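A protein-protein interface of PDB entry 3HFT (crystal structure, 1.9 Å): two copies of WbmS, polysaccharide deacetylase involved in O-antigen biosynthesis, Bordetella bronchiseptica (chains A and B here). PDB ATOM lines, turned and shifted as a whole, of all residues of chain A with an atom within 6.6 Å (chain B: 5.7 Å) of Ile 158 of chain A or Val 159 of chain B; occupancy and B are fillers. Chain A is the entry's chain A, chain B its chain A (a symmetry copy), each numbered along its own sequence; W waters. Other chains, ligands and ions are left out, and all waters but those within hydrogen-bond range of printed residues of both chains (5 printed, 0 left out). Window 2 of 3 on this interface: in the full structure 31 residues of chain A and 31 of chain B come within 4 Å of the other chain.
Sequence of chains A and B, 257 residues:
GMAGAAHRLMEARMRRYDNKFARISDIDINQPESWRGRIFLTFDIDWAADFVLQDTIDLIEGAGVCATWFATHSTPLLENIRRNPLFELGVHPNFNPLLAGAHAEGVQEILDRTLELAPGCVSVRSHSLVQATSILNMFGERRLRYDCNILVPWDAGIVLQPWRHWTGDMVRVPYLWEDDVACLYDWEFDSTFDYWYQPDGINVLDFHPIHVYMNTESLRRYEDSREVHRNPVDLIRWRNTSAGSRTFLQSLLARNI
The backbone carbonyl oxygen (O) of Ile 158 of chain A is in hydrogen-bond range of the side-chain amide nitrogen (NE2) of Gln 198 of chain A (3.0 Å). O of Ile 158 of chain B sits at hydrogen-bond distance from NE2 of Gln 198 of chain B. The backbone carbonyl oxygen of Asp 200 of chain B sits at hydrogen-bond distance from the side-chain amide nitrogen of Gln 161 of chain B (2.8 Å).
Among the printed residues, merely in contact across the chains: Pro 153 of chain A with Trp 163 of chain B (3.3 Å), Ile 158 of chain A with Ile 158 of chain B (3.3 Å), Ile 158 of chain A with Gln 161 of chain B (3.3 Å), Ile 158 of chain A with Val 159 of chain B (3.6 Å), Val 159 of chain A with Ile 158 of chain B (3.6 Å), Ala 156 of chain A with Trp 163 of chain B (3.6 Å), Ile 158 of chain A with Trp 163 of chain B (3.9 Å), Val 152 of chain A with Trp 163 of chain B (3.9 Å) and Ala 156 of chain A with Gln 161 of chain B (3.99 Å).
Of the printed residues of chain B, Val 152 of chain A touches Trp 163 (3.9 Å). Printed residues of chain B within 4 Å of Ala 156 of chain A: Gln 161 (3.99 Å) and Trp 163 (3.6 Å). Gly 157 of chain A touches none of the printed residues of chain B. Printed residues of chain B within 4 Å of Ile 158 of chain A: Ile 158, Val 159, Gln 161 and Trp 163. Of the printed residues of chain B, Val 159 of chain A touches Ile 158. Val 159 of chain B touches just one residue of chain A: Ile 158 (3.6 Å). Printed residues of chain A within 4 Å of Trp 163 of chain B: Val 152, Pro 153, Ala 156 and Ile 158. Gly 201 of chain B touches none of the printed residues of chain A. The nearest printed residue of chain B that does not touch Ile 158 of chain A is Leu 160 of chain B (4.6 Å). The nearest residue of chain A that does not touch Val 159 of chain B is Gly 157 of chain A (4.9 Å).
Of the 11 printed residues of chain B, 4 touch a printed residue of chain A. Hydrophobic or aromatic side chains of chain B that line the printed part of chain A: Ile 158 and Trp 163. Along chain B the printed residues that touch a printed residue of chain A span positions 158 to 163. Of the 11 printed residues of chain A, 5 touch a printed residue of chain B. Among the printed residues, 9 pairs touch across the chains. Among the printed residues, no Asp or Glu carboxylate lies within 4 Å of a Lys or Arg side-chain nitrogen of the other chain.
Ile 158 of chain A touches its own counterpart, Ile 158 of chain B. Ile 158 of chain A touches Val 159 of chain B, and with the chains exchanged Val 159 of chain A touches Ile 158 of chain B.
Water W4 lies within hydrogen-bond range of the backbone carbonyl oxygen (O) of Ala 156 of chain A (2.6 Å) and the backbone carbonyl oxygen (O) of Pro 162 of chain B (2.8 Å). Water W3 bridges the backbone carbonyl oxygen of Val 159 of chain A (2.7 Å) and the backbone carbonyl oxygen of Gly 157 of chain B (2.8 Å). Water W1 lies within hydrogen-bond range of O of Val 159 of chain B (2.7 Å), O of Gly 157 of chain A (2.8 Å) and NE2 of Gln 161 of chain B (3.0 Å). Water W2 lies within hydrogen-bond range of N of Val 159 of chain A (2.8 Å) and O of Val 159 of chain B (3.4 Å). Water W5 bridges the backbone NH of Val 159 of chain B (2.8 Å) and the backbone carbonyl oxygen of Val 159 of chain A (3.4 Å).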
ATOM      1  N   VAL A 152       5.852 -31.226  21.240  1.00  0.00           N
ATOM      2  CA  VAL A 152       5.427 -30.113  22.058  1.00  0.00           C
ATOM      3  C   VAL A 152       4.403 -30.670  23.047  1.00  0.00           C
ATOM      4  O   VAL A 152       3.328 -31.096  22.659  1.00  0.00           O
ATOM      5  CB  VAL A 152       4.765 -28.989  21.206  1.00  0.00           C
ATOM      6  CG1 VAL A 152       4.304 -27.868  22.131  1.00  0.00           C
ATOM      7  CG2 VAL A 152       5.746 -28.484  20.111  1.00  0.00           C
ATOM      8  N   PRO A 153       4.728 -30.674  24.335  1.00  0.00           N
ATOM      9  CA  PRO A 153       3.832 -31.295  25.310  1.00  0.00           C
ATOM     10  C   PRO A 153       2.421 -30.739  25.331  1.00  0.00           C
ATOM     11  O   PRO A 153       2.210 -29.531  25.211  1.00  0.00           O
ATOM     12  CB  PRO A 153       4.523 -31.026  26.653  1.00  0.00           C
ATOM     13  CG  PRO A 153       5.955 -30.788  26.307  1.00  0.00           C
ATOM     14  CD  PRO A 153       5.964 -30.156  24.944  1.00  0.00           C
ATOM     15  N   TRP A 154       1.456 -31.628  25.483  1.00  0.00           N
ATOM     16  CA  TRP A 154       0.049 -31.258  25.567  1.00  0.00           C
ATOM     17  C   TRP A 154      -0.259 -30.204  26.617  1.00  0.00           C
ATOM     18  O   TRP A 154      -1.281 -29.505  26.511  1.00  0.00           O
ATOM     19  CB  TRP A 154      -0.811 -32.514  25.863  1.00  0.00           C
ATOM     20  CG  TRP A 154      -0.602 -33.054  27.192  1.00  0.00           C
ATOM     21  CD1 TRP A 154       0.297 -34.014  27.559  1.00  0.00           C
ATOM     22  CD2 TRP A 154      -1.263 -32.651  28.388  1.00  0.00           C
ATOM     23  NE1 TRP A 154       0.220 -34.235  28.910  1.00  0.00           N
ATOM     24  CE2 TRP A 154      -0.716 -33.395  29.441  1.00  0.00           C
ATOM     25  CE3 TRP A 154      -2.258 -31.711  28.678  1.00  0.00           C
ATOM     26  CZ2 TRP A 154      -1.125 -33.243  30.742  1.00  0.00           C
ATOM     27  CZ3 TRP A 154      -2.676 -31.587  29.965  1.00  0.00           C
ATOM     28  CH2 TRP A 154      -2.107 -32.341  30.987  1.00  0.00           C
ATOM     29  N   ASP A 155       0.593 -30.097  27.637  1.00  0.00           N
ATOM     30  CA  ASP A 155       0.354 -29.173  28.740  1.00  0.00           C
ATOM     31  C   ASP A 155       1.189 -27.895  28.648  1.00  0.00           C
ATOM     32  O   ASP A 155       1.240 -27.111  29.591  1.00  0.00           O
ATOM     33  CB  ASP A 155       0.538 -29.850  30.102  1.00  0.00           C
ATOM     34  CG  ASP A 155       1.947 -30.361  30.337  1.00  0.00           C
ATOM     35  OD1 ASP A 155       2.726 -30.429  29.385  1.00  0.00           O
ATOM     36  OD2 ASP A 155       2.255 -30.731  31.504  1.00  0.00           O
ATOM     37  N   ALA A 156       1.825 -27.667  27.508  1.00  0.00           N
ATOM     38  CA  ALA A 156       2.603 -26.439  27.281  1.00  0.00           C
ATOM     39  C   ALA A 156       1.736 -25.191  27.028  1.00  0.00           C
ATOM     40  O   ALA A 156       2.243 -24.067  26.986  1.00  0.00           O
ATOM     41  CB  ALA A 156       3.611 -26.681  26.082  1.00  0.00           C
ATOM     42  N   GLY A 157       0.436 -25.375  26.807  1.00  0.00           N
ATOM     43  CA  GLY A 157      -0.498 -24.276  26.565  1.00  0.00           C
ATOM     44  C   GLY A 157      -0.537 -23.857  25.109  1.00  0.00           C
ATOM     45  O   GLY A 157      -0.916 -22.726  24.796  1.00  0.00           O
ATOM     46  N   ILE A 158      -0.089 -24.745  24.230  1.00  0.00           N
ATOM     47  CA  ILE A 158       0.049 -24.481  22.806  1.00  0.00           C
ATOM     48  C   ILE A 158      -0.887 -25.390  22.022  1.00  0.00           C
ATOM     49  O   ILE A 158      -0.790 -26.637  22.104  1.00  0.00           O
ATOM     50  CB  ILE A 158       1.502 -24.729  22.334  1.00  0.00           C
ATOM     51  CG1 ILE A 158       2.469 -23.793  23.090  1.00  0.00           C
ATOM     52  CG2 ILE A 158       1.608 -24.484  20.810  1.00  0.00           C
ATOM     53  CD1 ILE A 158       3.959 -24.120  22.936  1.00  0.00           C
ATOM     54  N   VAL A 159      -1.748 -24.768  21.225  1.00  0.00           N
ATOM     55  CA  VAL A 159      -2.623 -25.509  20.306  1.00  0.00           C
ATOM     56  C   VAL A 159      -1.817 -25.773  19.071  1.00  0.00           C
ATOM     57  O   VAL A 159      -1.309 -24.852  18.406  1.00  0.00           O
ATOM     58  CB  VAL A 159      -3.882 -24.752  19.956  1.00  0.00           C
ATOM     59  CG1 VAL A 159      -4.769 -25.542  18.964  1.00  0.00           C
ATOM     60  CG2 VAL A 159      -4.664 -24.434  21.222  1.00  0.00           C
ATOM     61  N   LEU A 160      -1.726 -27.051  18.732  1.00  0.00           N
ATOM     62  CA  LEU A 160      -0.825 -27.506  17.675  1.00  0.00           C
ATOM     63  C   LEU A 160      -1.478 -27.708  16.346  1.00  0.00           C
ATOM     64  O   LEU A 160      -2.661 -28.107  16.283  1.00  0.00           O
ATOM     65  CB  LEU A 160      -0.217 -28.799  18.089  1.00  0.00           C
ATOM     66  CG  LEU A 160       0.731 -28.744  19.289  1.00  0.00           C
ATOM     67  CD1 LEU A 160       1.146 -30.149  19.662  1.00  0.00           C
ATOM     68  CD2 LEU A 160       1.955 -27.842  18.968  1.00  0.00           C
ATOM     69  N   LEU A 176       2.169 -34.538  20.868  1.00  0.00           N
ATOM     70  CA  LEU A 176       1.919 -33.935  22.173  1.00  0.00           C
ATOM     71  C   LEU A 176       1.891 -34.863  23.406  1.00  0.00           C
ATOM     72  O   LEU A 176       1.777 -34.400  24.542  1.00  0.00           O
ATOM     73  CB  LEU A 176       0.606 -33.124  22.093  1.00  0.00           C
ATOM     74  CG  LEU A 176      -0.718 -33.750  21.599  1.00  0.00           C
ATOM     75  CD1 LEU A 176      -1.117 -35.041  22.348  1.00  0.00           C
ATOM     76  CD2 LEU A 176      -1.856 -32.695  21.629  1.00  0.00           C
ATOM     77  N   GLN A 198      -7.013 -31.753  21.989  1.00  0.00           N
ATOM     78  CA  GLN A 198      -7.258 -30.473  21.386  1.00  0.00           C
ATOM     79  C   GLN A 198      -8.333 -30.619  20.284  1.00  0.00           C
ATOM     80  O   GLN A 198      -8.062 -31.160  19.190  1.00  0.00           O
ATOM     81  CB  GLN A 198      -5.962 -29.934  20.768  1.00  0.00           C
ATOM     82  CG  GLN A 198      -4.755 -29.989  21.714  1.00  0.00           C
ATOM     83  CD  GLN A 198      -3.564 -29.225  21.205  1.00  0.00           C
ATOM     84  OE1 GLN A 198      -3.533 -28.784  20.042  1.00  0.00           O
ATOM     85  NE2 GLN A 198      -2.569 -29.035  22.087  1.00  0.00           N
ATOM     86  N   GLY B 157       0.289 -20.701  12.349  1.00  0.00           N
ATOM     87  CA  GLY B 157      -1.007 -20.560  13.014  1.00  0.00           C
ATOM     88  C   GLY B 157      -0.960 -20.983  14.469  1.00  0.00           C
ATOM     89  O   GLY B 157      -1.992 -21.329  15.050  1.00  0.00           O
ATOM     90  N   ILE B 158       0.240 -21.012  15.035  1.00  0.00           N
ATOM     91  CA  ILE B 158       0.491 -21.493  16.385  1.00  0.00           C
ATOM     92  C   ILE B 158       1.009 -20.351  17.248  1.00  0.00           C
ATOM     93  O   ILE B 158       2.064 -19.745  16.947  1.00  0.00           O
ATOM     94  CB  ILE B 158       1.536 -22.634  16.382  1.00  0.00           C
ATOM     95  CG1 ILE B 158       1.018 -23.820  15.540  1.00  0.00           C
ATOM     96  CG2 ILE B 158       1.815 -23.093  17.833  1.00  0.00           C
ATOM     97  CD1 ILE B 158       2.057 -24.900  15.214  1.00  0.00           C
ATOM     98  N   VAL B 159       0.301 -20.100  18.343  1.00  0.00           N
ATOM     99  CA  VAL B 159       0.748 -19.120  19.344  1.00  0.00           C
ATOM    100  C   VAL B 159       1.708 -19.839  20.243  1.00  0.00           C
ATOM    101  O   VAL B 159       1.381 -20.861  20.874  1.00  0.00           O
ATOM    102  CB  VAL B 159      -0.391 -18.544  20.150  1.00  0.00           C
ATOM    103  CG1 VAL B 159       0.111 -17.540  21.215  1.00  0.00           C
ATOM    104  CG2 VAL B 159      -1.392 -17.870  19.223  1.00  0.00           C
ATOM    105  N   LEU B 160       2.904 -19.277  20.337  1.00  0.00           N
ATOM    106  CA  LEU B 160       4.016 -19.943  21.012  1.00  0.00           C
ATOM    107  C   LEU B 160       4.242 -19.502  22.422  1.00  0.00           C
ATOM    108  O   LEU B 160       4.014 -18.319  22.753  1.00  0.00           O
ATOM    109  CB  LEU B 160       5.264 -19.683  20.244  1.00  0.00           C
ATOM    110  CG  LEU B 160       5.341 -20.307  18.851  1.00  0.00           C
ATOM    111  CD1 LEU B 160       6.599 -19.833  18.159  1.00  0.00           C
ATOM    112  CD2 LEU B 160       5.281 -21.856  18.950  1.00  0.00           C
ATOM    113  N   GLN B 161       4.728 -20.446  23.232  1.00  0.00           N
ATOM    114  CA  GLN B 161       5.036 -20.255  24.647  1.00  0.00           C
ATOM    115  C   GLN B 161       6.243 -21.174  24.960  1.00  0.00           C
ATOM    116  O   GLN B 161       6.316 -22.297  24.436  1.00  0.00           O
ATOM    117  CB  GLN B 161       3.829 -20.711  25.518  1.00  0.00           C
ATOM    118  CG  GLN B 161       2.414 -20.246  25.047  1.00  0.00           C
ATOM    119  CD  GLN B 161       2.161 -18.775  25.312  1.00  0.00           C
ATOM    120  OE1 GLN B 161       2.912 -18.162  26.058  1.00  0.00           O
ATOM    121  NE2 GLN B 161       1.090 -18.203  24.722  1.00  0.00           N
ATOM    122  N   PRO B 162       7.171 -20.741  25.836  1.00  0.00           N
ATOM    123  CA  PRO B 162       8.246 -21.651  26.214  1.00  0.00           C
ATOM    124  C   PRO B 162       7.614 -22.723  27.127  1.00  0.00           C
ATOM    125  O   PRO B 162       6.517 -22.521  27.644  1.00  0.00           O
ATOM    126  CB  PRO B 162       9.199 -20.747  27.019  1.00  0.00           C
ATOM    127  CG  PRO B 162       8.252 -19.768  27.663  1.00  0.00           C
ATOM    128  CD  PRO B 162       7.219 -19.498  26.611  1.00  0.00           C
ATOM    129  N   TRP B 163       8.287 -23.852  27.306  1.00  0.00           N
ATOM    130  CA  TRP B 163       7.787 -24.919  28.146  1.00  0.00           C
ATOM    131  C   TRP B 163       8.913 -25.639  28.876  1.00  0.00           C
ATOM    132  O   TRP B 163      10.075 -25.531  28.503  1.00  0.00           O
ATOM    133  CB  TRP B 163       6.934 -25.899  27.319  1.00  0.00           C
ATOM    134  CG  TRP B 163       7.619 -26.729  26.324  1.00  0.00           C
ATOM    135  CD1 TRP B 163       8.208 -27.932  26.556  1.00  0.00           C
ATOM    136  CD2 TRP B 163       7.779 -26.474  24.911  1.00  0.00           C
ATOM    137  NE1 TRP B 163       8.722 -28.435  25.404  1.00  0.00           N
ATOM    138  CE2 TRP B 163       8.466 -27.572  24.373  1.00  0.00           C
ATOM    139  CE3 TRP B 163       7.417 -25.425  24.069  1.00  0.00           C
ATOM    140  CZ2 TRP B 163       8.799 -27.660  23.037  1.00  0.00           C
ATOM    141  CZ3 TRP B 163       7.733 -25.500  22.744  1.00  0.00           C
ATOM    142  CH2 TRP B 163       8.434 -26.615  22.224  1.00  0.00           C
ATOM    143  N   PRO B 174      10.809 -21.831  21.862  1.00  0.00           N
ATOM    144  CA  PRO B 174      10.670 -21.937  20.415  1.00  0.00           C
ATOM    145  C   PRO B 174      10.824 -20.564  19.761  1.00  0.00           C
ATOM    146  O   PRO B 174      10.460 -19.561  20.368  1.00  0.00           O
ATOM    147  CB  PRO B 174       9.237 -22.415  20.253  1.00  0.00           C
ATOM    148  CG  PRO B 174       8.515 -21.737  21.368  1.00  0.00           C
ATOM    149  CD  PRO B 174       9.501 -21.796  22.525  1.00  0.00           C
ATOM    150  N   GLN B 198       3.301 -11.855  18.010  1.00  0.00           N
ATOM    151  CA  GLN B 198       2.293 -12.438  18.851  1.00  0.00           C
ATOM    152  C   GLN B 198       2.203 -11.643  20.174  1.00  0.00           C
ATOM    153  O   GLN B 198       3.091 -11.747  21.048  1.00  0.00           O
ATOM    154  CB  GLN B 198       2.653 -13.898  19.154  1.00  0.00           C
ATOM    155  CG  GLN B 198       3.017 -14.718  17.909  1.00  0.00           C
ATOM    156  CD  GLN B 198       3.109 -16.195  18.175  1.00  0.00           C
ATOM    157  OE1 GLN B 198       3.088 -16.642  19.336  1.00  0.00           O
ATOM    158  NE2 GLN B 198       3.186 -16.982  17.089  1.00  0.00           N
ATOM    159  N   ASP B 200       0.332 -12.279  22.375  1.00  0.00           N
ATOM    160  CA  ASP B 200      -0.071 -13.328  23.305  1.00  0.00           C
ATOM    161  C   ASP B 200       0.897 -14.518  23.373  1.00  0.00           C
ATOM    162  O   ASP B 200       0.583 -15.522  24.010  1.00  0.00           O
ATOM    163  CB  ASP B 200      -1.465 -13.874  22.947  1.00  0.00           C
ATOM    164  CG  ASP B 200      -1.628 -14.214  21.449  1.00  0.00           C
ATOM    165  OD1 ASP B 200      -0.738 -13.946  20.615  1.00  0.00           O
ATOM    166  OD2 ASP B 200      -2.712 -14.722  21.108  1.00  0.00           O
ATOM    167  N   GLY B 201       2.059 -14.386  22.765  1.00  0.00           N
ATOM    168  CA  GLY B 201       3.039 -15.465  22.771  1.00  0.00           C
ATOM    169  C   GLY B 201       4.428 -14.918  22.929  1.00  0.00           C
ATOM    170  O   GLY B 201       4.611 -13.704  23.128  1.00  0.00           O
HETATM  171  O   HOH W   1      -0.023 -20.598  23.208  1.00  0.00           O
HETATM  172  O   HOH W   2      -1.841 -21.920  21.231  1.00  0.00           O
HETATM  173  O   HOH W   3      -2.868 -23.466  16.635  1.00  0.00           O
HETATM  174  O   HOH W   4       4.130 -23.507  28.633  1.00  0.00           O
HETATM  175  O   HOH W   5      -2.101 -21.560  18.812  1.00  0.00           O
